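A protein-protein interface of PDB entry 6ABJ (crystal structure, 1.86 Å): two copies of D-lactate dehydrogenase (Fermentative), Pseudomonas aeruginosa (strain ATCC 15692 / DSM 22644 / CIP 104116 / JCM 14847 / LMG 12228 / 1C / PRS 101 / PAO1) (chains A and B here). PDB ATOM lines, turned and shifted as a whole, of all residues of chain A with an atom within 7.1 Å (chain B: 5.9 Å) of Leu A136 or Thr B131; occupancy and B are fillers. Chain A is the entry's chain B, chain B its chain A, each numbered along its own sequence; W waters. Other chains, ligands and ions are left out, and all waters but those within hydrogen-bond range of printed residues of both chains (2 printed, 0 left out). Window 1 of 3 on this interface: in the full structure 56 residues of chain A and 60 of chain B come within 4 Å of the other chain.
Gly A127 touches Leu B130, and with the chains exchanged Leu A130 touches Gly B127. Gly A127 touches Leu B136, and with the chains exchanged Leu A136 touches Gly B127. Leu B130 touches its own counterpart, Leu A130. Leu A136 touches Thr B131, but with the chains exchanged Thr A131 does not touch Leu B136 (4.2 Å). Of the 14 pairs that touch across the chains among the printed residues, 5 have their exchanged pair printed and touching as well.
Of the 15 printed residues of chain A, 7 touch a printed residue of chain B. Hydrophobic or aromatic side chains of chain A that line the printed part of chain B: Leu A130, Leu A136, Ala A139, Tyr A140 and Leu A153. Among the printed residues, 14 pairs touch across the chains. Among the printed residues, no Asp or Glu carboxylate lies within 4 Å of a Lys or Arg side-chain nitrogen of the other chain.
The backbone carbonyl oxygen (O) of Arg A134 lies within hydrogen-bond range of the side-chain amide nitrogen (NE2) of Gln B312 (2.8 Å). ND1 of His B124 is in hydrogen-bond range of NH2 of Arg A134 (3.4 Å).
A ring nitrogen (NE2) of His B124 sits at hydrogen-bond distance from the side-chain hydroxyl of Thr B309 (2.8 Å). The backbone NH (N) of Leu A136 lies within hydrogen-bond range of the backbone carbonyl oxygen (O) of Thr A131. The side-chain hydroxyl (OG1) of Thr B131 sits at hydrogen-bond distance from the backbone carbonyl oxygen (O) of Gly B127 (2.7 Å). The backbone carbonyl oxygen (O) of Thr B131 lies close to a ring nitrogen (ND1) of His B137. The backbone carbonyl oxygen of Thr B131 lies within hydrogen-bond range of the backbone NH of Leu B136.
Among the printed residues, pairs that only touch across the chains: Leu A136 with Thr B131 (3.2 Å), Gly A127 with Leu B136 (3.4 Å), Leu A136 with Gly B127 (3.4 Å), Ala A139 with Gln B312 (3.5 Å), Leu A153 with Gln B312 (3.5 Å), Tyr A140 with His B137 (3.6 Å), Leu A136 with His B124 (3.7 Å), Gly A127 with Leu B130 (3.8 Å), Leu A130 with Gly B127 (3.8 Å), Leu A130 with Val B126 (3.8 Å), Leu A130 with Leu B130 (3.9 Å) and Ala A139 with Thr B309 (3.98 Å).
Water W1 lies within hydrogen-bond range of O of Leu A153 (2.7 Å), NE of Arg A134 (3.0 Å) and NE2 of Gln B312 (3.1 Å). Water W2 lies within hydrogen-bond range of O of His A137 (2.9 Å), O of His B137 (2.9 Å) and ND2 of Asn A141 (3.4 Å).
Of the printed residues of chain B, Gly A127 touches Leu B130 and Leu B136. Of the printed residues of chain B, Leu A130 touches Val B126 (3.8 Å), Gly B127 (3.8 Å) and Leu B130 (3.9 Å). Printed residues of chain B within 4 Å of Arg A134: His B124 (3.4 Å) and Gln B312 (2.8 Å). Leu A136 touches just these residues of chain B: His B124, Gly B127 and Thr B131. Printed residues of chain B within 4 Å of Leu A153: Gln B312. Of the printed residues of chain A, Thr B131 touches Leu A136. Asn B133 touches none of the printed residues of chain A. Printed residues of chain A within 4 Å of Thr B309: Ala A139 (3.98 Å). The nearest residue of chain B that does not touch Leu A136 is Leu B128 (4.1 Å). The nearest residue of chain A that does not touch Thr B131 is Thr A131 (4.4 Å).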
ATOM      1  N   GLY A 127     -12.081 -20.414   1.635  1.00  0.00           N
ATOM      2  CA  GLY A 127     -11.854 -21.621   2.379  1.00  0.00           C
ATOM      3  C   GLY A 127     -12.078 -22.888   1.520  1.00  0.00           C
ATOM      4  O   GLY A 127     -11.308 -23.862   1.584  1.00  0.00           O
ATOM      5  N   LEU A 130      -9.043 -23.327  -0.739  1.00  0.00           N
ATOM      6  CA  LEU A 130      -7.840 -23.831  -0.101  1.00  0.00           C
ATOM      7  C   LEU A 130      -7.984 -25.258   0.323  1.00  0.00           C
ATOM      8  O   LEU A 130      -7.062 -26.029   0.180  1.00  0.00           O
ATOM      9  CB  LEU A 130      -7.463 -22.964   1.101  1.00  0.00           C
ATOM     10  CG  LEU A 130      -6.708 -21.694   0.643  1.00  0.00           C
ATOM     11  CD1 LEU A 130      -6.781 -20.692   1.731  1.00  0.00           C
ATOM     12  CD2 LEU A 130      -5.277 -22.032   0.198  1.00  0.00           C
ATOM     13  N   THR A 131      -9.177 -25.652   0.799  1.00  0.00           N
ATOM     14  CA  THR A 131      -9.352 -27.017   1.171  1.00  0.00           C
ATOM     15  C   THR A 131      -9.222 -27.943  -0.063  1.00  0.00           C
ATOM     16  O   THR A 131      -8.659 -29.034   0.029  1.00  0.00           O
ATOM     17  CB  THR A 131     -10.641 -27.314   2.012  1.00  0.00           C
ATOM     18  OG1 THR A 131     -10.558 -28.679   2.465  1.00  0.00           O
ATOM     19  CG2 THR A 131     -11.853 -27.258   1.242  1.00  0.00           C
ATOM     20  N   LEU A 132      -9.810 -27.537  -1.170  1.00  0.00           N
ATOM     21  CA  LEU A 132      -9.718 -28.330  -2.366  1.00  0.00           C
ATOM     22  C   LEU A 132      -8.261 -28.400  -2.889  1.00  0.00           C
ATOM     23  O   LEU A 132      -7.773 -29.458  -3.260  1.00  0.00           O
ATOM     24  CB  LEU A 132     -10.605 -27.745  -3.461  1.00  0.00           C
ATOM     25  CG  LEU A 132     -12.131 -27.979  -3.317  1.00  0.00           C
ATOM     26  CD1 LEU A 132     -12.915 -27.004  -4.172  1.00  0.00           C
ATOM     27  CD2 LEU A 132     -12.399 -29.439  -3.724  1.00  0.00           C
ATOM     28  N   ASN A 133      -7.601 -27.243  -2.886  1.00  0.00           N
ATOM     29  CA  ASN A 133      -6.265 -27.119  -3.453  1.00  0.00           C
ATOM     30  C   ASN A 133      -5.302 -28.034  -2.650  1.00  0.00           C
ATOM     31  O   ASN A 133      -4.593 -28.881  -3.218  1.00  0.00           O
ATOM     32  CB  ASN A 133      -5.863 -25.673  -3.333  1.00  0.00           C
ATOM     33  CG  ASN A 133      -4.483 -25.374  -3.873  1.00  0.00           C
ATOM     34  OD1 ASN A 133      -3.585 -26.241  -3.878  1.00  0.00           O
ATOM     35  ND2 ASN A 133      -4.269 -24.117  -4.224  1.00  0.00           N
ATOM     36  N   ARG A 134      -5.324 -27.877  -1.332  1.00  0.00           N
ATOM     37  CA  ARG A 134      -4.394 -28.554  -0.474  1.00  0.00           C
ATOM     38  C   ARG A 134      -4.993 -29.920   0.057  1.00  0.00           C
ATOM     39  O   ARG A 134      -4.372 -30.615   0.883  1.00  0.00           O
ATOM     40  CB  ARG A 134      -3.889 -27.675   0.657  1.00  0.00           C
ATOM     41  CG  ARG A 134      -3.393 -26.281   0.207  1.00  0.00           C
ATOM     42  CD  ARG A 134      -2.316 -26.388  -0.867  1.00  0.00           C
ATOM     43  NE  ARG A 134      -1.132 -26.891  -0.277  1.00  0.00           N
ATOM     44  CZ  ARG A 134      -0.104 -26.168   0.180  1.00  0.00           C
ATOM     45  NH1 ARG A 134      -0.001 -24.881  -0.027  1.00  0.00           N
ATOM     46  NH2 ARG A 134       0.880 -26.783   0.758  1.00  0.00           N
ATOM     47  N   ARG A 135      -6.186 -30.253  -0.415  1.00  0.00           N
ATOM     48  CA  ARG A 135      -6.831 -31.494  -0.021  1.00  0.00           C
ATOM     49  C   ARG A 135      -6.929 -31.643   1.482  1.00  0.00           C
ATOM     50  O   ARG A 135      -6.738 -32.734   2.021  1.00  0.00           O
ATOM     51  CB  ARG A 135      -6.071 -32.689  -0.600  1.00  0.00           C
ATOM     52  CG  ARG A 135      -6.298 -32.906  -2.084  1.00  0.00           C
ATOM     53  CD  ARG A 135      -5.332 -32.067  -2.901  1.00  0.00           C
ATOM     54  NE  ARG A 135      -5.018 -32.691  -4.181  1.00  0.00           N
ATOM     55  CZ  ARG A 135      -4.774 -32.014  -5.298  1.00  0.00           C
ATOM     56  NH1 ARG A 135      -4.806 -30.689  -5.290  1.00  0.00           N
ATOM     57  NH2 ARG A 135      -4.497 -32.661  -6.422  1.00  0.00           N
ATOM     58  N   LEU A 136      -7.234 -30.548   2.159  1.00  0.00           N
ATOM     59  CA  LEU A 136      -7.200 -30.549   3.595  1.00  0.00           C
ATOM     60  C   LEU A 136      -8.250 -31.495   4.252  1.00  0.00           C
ATOM     61  O   LEU A 136      -7.983 -32.052   5.268  1.00  0.00           O
ATOM     62  CB  LEU A 136      -7.419 -29.166   4.128  1.00  0.00           C
ATOM     63  CG  LEU A 136      -6.352 -28.087   3.730  1.00  0.00           C
ATOM     64  CD1 LEU A 136      -6.680 -26.695   4.233  1.00  0.00           C
ATOM     65  CD2 LEU A 136      -4.977 -28.564   4.130  1.00  0.00           C
ATOM     66  N   HIS A 137      -9.400 -31.631   3.624  1.00  0.00           N
ATOM     67  CA  HIS A 137     -10.470 -32.539   4.113  1.00  0.00           C
ATOM     68  C   HIS A 137      -9.969 -33.987   4.013  1.00  0.00           C
ATOM     69  O   HIS A 137     -10.157 -34.796   4.951  1.00  0.00           O
ATOM     70  CB  HIS A 137     -11.743 -32.271   3.285  1.00  0.00           C
ATOM     71  CG  HIS A 137     -11.590 -32.457   1.815  1.00  0.00           C
ATOM     72  ND1 HIS A 137     -10.859 -31.623   1.008  1.00  0.00           N
ATOM     73  CD2 HIS A 137     -12.075 -33.401   0.997  1.00  0.00           C
ATOM     74  CE1 HIS A 137     -10.905 -32.043  -0.227  1.00  0.00           C
ATOM     75  NE2 HIS A 137     -11.661 -33.118  -0.258  1.00  0.00           N
ATOM     76  N   ARG A 138      -9.250 -34.299   2.942  1.00  0.00           N
ATOM     77  CA  ARG A 138      -8.655 -35.663   2.777  1.00  0.00           C
ATOM     78  C   ARG A 138      -7.509 -35.879   3.791  1.00  0.00           C
ATOM     79  O   ARG A 138      -7.411 -36.938   4.421  1.00  0.00           O
ATOM     80  CB  ARG A 138      -8.160 -35.875   1.386  1.00  0.00           C
ATOM     81  CG  ARG A 138      -9.297 -35.718   0.315  1.00  0.00           C
ATOM     82  CD  ARG A 138      -8.848 -36.243  -1.082  1.00  0.00           C
ATOM     83  NE  ARG A 138      -8.552 -37.671  -1.015  1.00  0.00           N
ATOM     84  CZ  ARG A 138      -7.601 -38.308  -1.705  1.00  0.00           C
ATOM     85  NH1 ARG A 138      -6.866 -37.669  -2.626  1.00  0.00           N
ATOM     86  NH2 ARG A 138      -7.439 -39.606  -1.487  1.00  0.00           N
ATOM     87  N   ALA A 139      -6.627 -34.868   3.919  1.00  0.00           N
ATOM     88  CA  ALA A 139      -5.533 -34.949   4.930  1.00  0.00           C
ATOM     89  C   ALA A 139      -6.023 -35.197   6.339  1.00  0.00           C
ATOM     90  O   ALA A 139      -5.499 -36.026   7.045  1.00  0.00           O
ATOM     91  CB  ALA A 139      -4.681 -33.719   4.874  1.00  0.00           C
ATOM     92  N   TYR A 140      -7.041 -34.445   6.754  1.00  0.00           N
ATOM     93  CA  TYR A 140      -7.597 -34.571   8.078  1.00  0.00           C
ATOM     94  C   TYR A 140      -7.996 -35.975   8.335  1.00  0.00           C
ATOM     95  O   TYR A 140      -7.681 -36.561   9.399  1.00  0.00           O
ATOM     96  CB  TYR A 140      -8.829 -33.599   8.239  1.00  0.00           C
ATOM     97  CG  TYR A 140      -9.546 -33.811   9.469  1.00  0.00           C
ATOM     98  CD1 TYR A 140      -9.012 -33.411  10.680  1.00  0.00           C
ATOM     99  CD2 TYR A 140     -10.803 -34.402   9.458  1.00  0.00           C
ATOM    100  CE1 TYR A 140      -9.695 -33.610  11.881  1.00  0.00           C
ATOM    101  CE2 TYR A 140     -11.468 -34.671  10.616  1.00  0.00           C
ATOM    102  CZ  TYR A 140     -10.937 -34.228  11.836  1.00  0.00           C
ATOM    103  OH  TYR A 140     -11.598 -34.508  12.980  1.00  0.00           O
ATOM    104  N   ASN A 141      -8.726 -36.557   7.371  1.00  0.00           N
ATOM    105  CA  ASN A 141      -9.195 -37.915   7.553  1.00  0.00           C
ATOM    106  C   ASN A 141      -8.067 -38.955   7.617  1.00  0.00           C
ATOM    107  O   ASN A 141      -8.193 -39.926   8.291  1.00  0.00           O
ATOM    108  CB  ASN A 141     -10.220 -38.269   6.461  1.00  0.00           C
ATOM    109  CG  ASN A 141     -11.587 -37.597   6.725  1.00  0.00           C
ATOM    110  OD1 ASN A 141     -11.984 -37.327   7.873  1.00  0.00           O
ATOM    111  ND2 ASN A 141     -12.285 -37.322   5.673  1.00  0.00           N
ATOM    112  N   ARG A 142      -6.985 -38.710   6.912  1.00  0.00           N
ATOM    113  CA  ARG A 142      -5.825 -39.549   7.039  1.00  0.00           C
ATOM    114  C   ARG A 142      -5.145 -39.417   8.364  1.00  0.00           C
ATOM    115  O   ARG A 142      -4.970 -40.379   9.099  1.00  0.00           O
ATOM    116  CB  ARG A 142      -4.791 -39.247   5.935  1.00  0.00           C
ATOM    117  CG  ARG A 142      -5.244 -39.691   4.543  1.00  0.00           C
ATOM    118  CD  ARG A 142      -4.076 -39.490   3.613  1.00  0.00           C
ATOM    119  NE  ARG A 142      -4.485 -39.647   2.238  1.00  0.00           N
ATOM    120  CZ  ARG A 142      -3.693 -39.503   1.174  1.00  0.00           C
ATOM    121  NH1 ARG A 142      -2.401 -39.152   1.310  1.00  0.00           N
ATOM    122  NH2 ARG A 142      -4.228 -39.653  -0.038  1.00  0.00           N
ATOM    123  N   LEU A 153      -1.887 -35.621  -2.294  1.00  0.00           N
ATOM    124  CA  LEU A 153      -2.252 -34.382  -1.623  1.00  0.00           C
ATOM    125  C   LEU A 153      -1.573 -33.107  -2.170  1.00  0.00           C
ATOM    126  O   LEU A 153      -1.869 -32.003  -1.706  1.00  0.00           O
ATOM    127  CB  LEU A 153      -1.957 -34.491  -0.128  1.00  0.00           C
ATOM    128  CG  LEU A 153      -2.566 -35.653   0.617  1.00  0.00           C
ATOM    129  CD1 LEU A 153      -2.258 -35.555   2.105  1.00  0.00           C
ATOM    130  CD2 LEU A 153      -4.108 -35.700   0.448  1.00  0.00           C
ATOM    131  N   HIS B 124      -0.676 -22.555   2.968  1.00  0.00           N
ATOM    132  CA  HIS B 124      -1.100 -23.723   3.740  1.00  0.00           C
ATOM    133  C   HIS B 124      -1.571 -23.291   5.111  1.00  0.00           C
ATOM    134  O   HIS B 124      -2.572 -23.769   5.596  1.00  0.00           O
ATOM    135  CB  HIS B 124       0.022 -24.733   3.822  1.00  0.00           C
ATOM    136  CG  HIS B 124      -0.385 -26.074   4.326  1.00  0.00           C
ATOM    137  ND1 HIS B 124      -1.115 -26.964   3.557  1.00  0.00           N
ATOM    138  CD2 HIS B 124      -0.262 -26.653   5.554  1.00  0.00           C
ATOM    139  CE1 HIS B 124      -1.327 -28.077   4.252  1.00  0.00           C
ATOM    140  NE2 HIS B 124      -0.899 -27.885   5.491  1.00  0.00           N
ATOM    141  N   VAL B 126      -2.856 -20.419   5.901  1.00  0.00           N
ATOM    142  CA  VAL B 126      -4.159 -19.772   5.744  1.00  0.00           C
ATOM    143  C   VAL B 126      -5.239 -20.825   5.517  1.00  0.00           C
ATOM    144  O   VAL B 126      -6.372 -20.709   6.009  1.00  0.00           O
ATOM    145  CB  VAL B 126      -4.134 -18.774   4.648  1.00  0.00           C
ATOM    146  CG1 VAL B 126      -5.515 -18.225   4.397  1.00  0.00           C
ATOM    147  CG2 VAL B 126      -3.148 -17.642   4.985  1.00  0.00           C
ATOM    148  N   GLY B 127      -4.911 -21.892   4.768  1.00  0.00           N
ATOM    149  CA  GLY B 127      -5.884 -22.957   4.607  1.00  0.00           C
ATOM    150  C   GLY B 127      -6.283 -23.649   5.903  1.00  0.00           C
ATOM    151  O   GLY B 127      -7.485 -23.986   6.092  1.00  0.00           O
ATOM    152  N   LEU B 128      -5.309 -23.848   6.784  1.00  0.00           N
ATOM    153  CA  LEU B 128      -5.536 -24.461   8.049  1.00  0.00           C
ATOM    154  C   LEU B 128      -6.473 -23.506   8.839  1.00  0.00           C
ATOM    155  O   LEU B 128      -7.444 -23.966   9.471  1.00  0.00           O
ATOM    156  CB  LEU B 128      -4.224 -24.724   8.810  1.00  0.00           C
ATOM    157  CG  LEU B 128      -3.319 -25.866   8.352  1.00  0.00           C
ATOM    158  CD1 LEU B 128      -2.060 -25.917   9.139  1.00  0.00           C
ATOM    159  CD2 LEU B 128      -4.101 -27.188   8.443  1.00  0.00           C
ATOM    160  N   ILE B 129      -6.202 -22.216   8.759  1.00  0.00           N
ATOM    161  CA  ILE B 129      -7.082 -21.230   9.413  1.00  0.00           C
ATOM    162  C   ILE B 129      -8.540 -21.359   8.989  1.00  0.00           C
ATOM    163  O   ILE B 129      -9.455 -21.424   9.818  1.00  0.00           O
ATOM    164  CB  ILE B 129      -6.585 -19.805   9.228  1.00  0.00           C
ATOM    165  CG1 ILE B 129      -5.307 -19.629  10.030  1.00  0.00           C
ATOM    166  CG2 ILE B 129      -7.602 -18.784   9.672  1.00  0.00           C
ATOM    167  CD1 ILE B 129      -4.543 -18.355   9.781  1.00  0.00           C
ATOM    168  N   LEU B 130      -8.755 -21.364   7.675  1.00  0.00           N
ATOM    169  CA  LEU B 130     -10.045 -21.338   7.187  1.00  0.00           C
ATOM    170  C   LEU B 130     -10.752 -22.652   7.477  1.00  0.00           C
ATOM    171  O   LEU B 130     -11.954 -22.672   7.759  1.00  0.00           O
ATOM    172  CB  LEU B 130     -10.056 -20.989   5.681  1.00  0.00           C
ATOM    173  CG  LEU B 130      -9.963 -19.464   5.471  1.00  0.00           C
ATOM    174  CD1 LEU B 130      -9.521 -19.173   4.079  1.00  0.00           C
ATOM    175  CD2 LEU B 130     -11.269 -18.762   5.810  1.00  0.00           C
ATOM    176  N   THR B 131     -10.051 -23.793   7.346  1.00  0.00           N
ATOM    177  CA  THR B 131     -10.697 -25.036   7.609  1.00  0.00           C
ATOM    178  C   THR B 131     -11.145 -25.191   9.045  1.00  0.00           C
ATOM    179  O   THR B 131     -12.243 -25.704   9.320  1.00  0.00           O
ATOM    180  CB  THR B 131      -9.788 -26.241   7.273  1.00  0.00           C
ATOM    181  OG1 THR B 131      -9.254 -26.031   5.950  1.00  0.00           O
ATOM    182  CG2 THR B 131     -10.667 -27.414   7.237  1.00  0.00           C
ATOM    183  N   LEU B 132     -10.313 -24.714   9.960  1.00  0.00           N
ATOM    184  CA  LEU B 132     -10.689 -24.728  11.398  1.00  0.00           C
ATOM    185  C   LEU B 132     -11.845 -23.766  11.690  1.00  0.00           C
ATOM    186  O   LEU B 132     -12.768 -24.119  12.381  1.00  0.00           O
ATOM    187  CB  LEU B 132      -9.489 -24.331  12.243  1.00  0.00           C
ATOM    188  CG  LEU B 132      -8.370 -25.360  12.398  1.00  0.00           C
ATOM    189  CD1 LEU B 132      -7.041 -24.736  12.793  1.00  0.00           C
ATOM    190  CD2 LEU B 132      -8.826 -26.406  13.379  1.00  0.00           C
ATOM    191  N   ASN B 133     -11.775 -22.570  11.131  1.00  0.00           N
ATOM    192  CA  ASN B 133     -12.785 -21.517  11.382  1.00  0.00           C
ATOM    193  C   ASN B 133     -14.143 -21.994  10.904  1.00  0.00           C
ATOM    194  O   ASN B 133     -15.122 -21.963  11.632  1.00  0.00           O
ATOM    195  CB  ASN B 133     -12.326 -20.281  10.631  1.00  0.00           C
ATOM    196  CG  ASN B 133     -13.233 -19.088  10.777  1.00  0.00           C
ATOM    197  OD1 ASN B 133     -14.399 -19.216  11.021  1.00  0.00           O
ATOM    198  ND2 ASN B 133     -12.664 -17.914  10.613  1.00  0.00           N
ATOM    199  N   ARG B 134     -14.182 -22.407   9.649  1.00  0.00           N
ATOM    200  CA  ARG B 134     -15.440 -22.778   9.054  1.00  0.00           C
ATOM    201  C   ARG B 134     -15.770 -24.254   9.185  1.00  0.00           C
ATOM    202  O   ARG B 134     -16.774 -24.725   8.647  1.00  0.00           O
ATOM    203  CB  ARG B 134     -15.480 -22.345   7.581  1.00  0.00           C
ATOM    204  CG  ARG B 134     -15.108 -20.886   7.344  1.00  0.00           C
ATOM    205  CD  ARG B 134     -15.987 -19.952   8.162  1.00  0.00           C
ATOM    206  NE  ARG B 134     -17.348 -19.926   7.639  1.00  0.00           N
ATOM    207  CZ  ARG B 134     -17.837 -18.962   6.865  1.00  0.00           C
ATOM    208  NH1 ARG B 134     -17.080 -17.927   6.531  1.00  0.00           N
ATOM    209  NH2 ARG B 134     -19.084 -19.033   6.429  1.00  0.00           N
ATOM    210  N   ARG B 135     -14.923 -24.974   9.908  1.00  0.00           N
ATOM    211  CA  ARG B 135     -15.145 -26.395  10.160  1.00  0.00           C
ATOM    212  C   ARG B 135     -15.354 -27.182   8.894  1.00  0.00           C
ATOM    213  O   ARG B 135     -16.216 -28.058   8.818  1.00  0.00           O
ATOM    214  CB  ARG B 135     -16.343 -26.593  11.089  1.00  0.00           C
ATOM    215  CG  ARG B 135     -16.041 -26.303  12.546  1.00  0.00           C
ATOM    216  CD  ARG B 135     -16.223 -24.830  12.847  1.00  0.00           C
ATOM    217  NE  ARG B 135     -16.538 -24.617  14.252  1.00  0.00           N
ATOM    218  CZ  ARG B 135     -16.235 -23.513  14.923  1.00  0.00           C
ATOM    219  NH1 ARG B 135     -15.609 -22.517  14.313  1.00  0.00           N
ATOM    220  NH2 ARG B 135     -16.557 -23.404  16.204  1.00  0.00           N
ATOM    221  N   LEU B 136     -14.546 -26.867   7.898  1.00  0.00           N
ATOM    222  CA  LEU B 136     -14.745 -27.424   6.589  1.00  0.00           C
ATOM    223  C   LEU B 136     -14.480 -28.971   6.502  1.00  0.00           C
ATOM    224  O   LEU B 136     -15.165 -29.654   5.769  1.00  0.00           O
ATOM    225  CB  LEU B 136     -13.853 -26.750   5.544  1.00  0.00           C
ATOM    226  CG  LEU B 136     -14.077 -25.265   5.300  1.00  0.00           C
ATOM    227  CD1 LEU B 136     -13.140 -24.637   4.301  1.00  0.00           C
ATOM    228  CD2 LEU B 136     -15.529 -25.000   4.973  1.00  0.00           C
ATOM    229  N   HIS B 137     -13.570 -29.433   7.320  1.00  0.00           N
ATOM    230  CA  HIS B 137     -13.267 -30.830   7.412  1.00  0.00           C
ATOM    231  C   HIS B 137     -14.443 -31.592   7.989  1.00  0.00           C
ATOM    232  O   HIS B 137     -14.814 -32.632   7.511  1.00  0.00           O
ATOM    233  CB  HIS B 137     -11.976 -31.021   8.184  1.00  0.00           C
ATOM    234  CG  HIS B 137     -11.987 -30.412   9.549  1.00  0.00           C
ATOM    235  ND1 HIS B 137     -11.921 -29.117   9.752  1.00  0.00           N
ATOM    236  CD2 HIS B 137     -12.029 -30.985  10.775  1.00  0.00           C
ATOM    237  CE1 HIS B 137     -11.967 -28.870  11.046  1.00  0.00           C
ATOM    238  NE2 HIS B 137     -12.025 -30.017  11.674  1.00  0.00           N
ATOM    239  N   VAL B 307      -6.729 -29.637  13.548  1.00  0.00           N
ATOM    240  CA  VAL B 307      -6.356 -30.242  12.293  1.00  0.00           C
ATOM    241  C   VAL B 307      -4.853 -30.356  12.242  1.00  0.00           C
ATOM    242  O   VAL B 307      -4.127 -29.369  12.414  1.00  0.00           O
ATOM    243  CB  VAL B 307      -6.860 -29.428  11.109  1.00  0.00           C
ATOM    244  CG1 VAL B 307      -6.284 -29.988   9.802  1.00  0.00           C
ATOM    245  CG2 VAL B 307      -8.368 -29.406  11.136  1.00  0.00           C
ATOM    246  N   THR B 309      -1.766 -31.612   9.611  1.00  0.00           N
ATOM    247  CA  THR B 309      -1.309 -32.099   8.332  1.00  0.00           C
ATOM    248  C   THR B 309       0.109 -32.549   8.524  1.00  0.00           C
ATOM    249  O   THR B 309       0.868 -31.978   9.378  1.00  0.00           O
ATOM    250  CB  THR B 309      -1.488 -31.041   7.206  1.00  0.00           C
ATOM    251  OG1 THR B 309      -0.866 -29.827   7.573  1.00  0.00           O
ATOM    252  CG2 THR B 309      -2.906 -30.812   6.928  1.00  0.00           C
ATOM    253  N   GLN B 312       3.077 -31.047   5.178  1.00  0.00           N
ATOM    254  CA  GLN B 312       2.526 -30.922   3.866  1.00  0.00           C
ATOM    255  C   GLN B 312       2.583 -29.470   3.321  1.00  0.00           C
ATOM    256  O   GLN B 312       2.129 -29.202   2.198  1.00  0.00           O
ATOM    257  CB  GLN B 312       1.048 -31.343   4.021  1.00  0.00           C
ATOM    258  CG  GLN B 312       0.328 -31.651   2.769  1.00  0.00           C
ATOM    259  CD  GLN B 312      -1.163 -31.845   2.977  1.00  0.00           C
ATOM    260  OE1 GLN B 312      -1.565 -32.600   3.830  1.00  0.00           O
ATOM    261  NE2 GLN B 312      -1.967 -31.279   2.076  1.00  0.00           N
HETATM  262  O   HOH W   1      -0.824 -29.880  -0.453  1.00  0.00           O
HETATM  263  O   HOH W   2     -12.536 -34.046   6.363  1.00  0.00           O
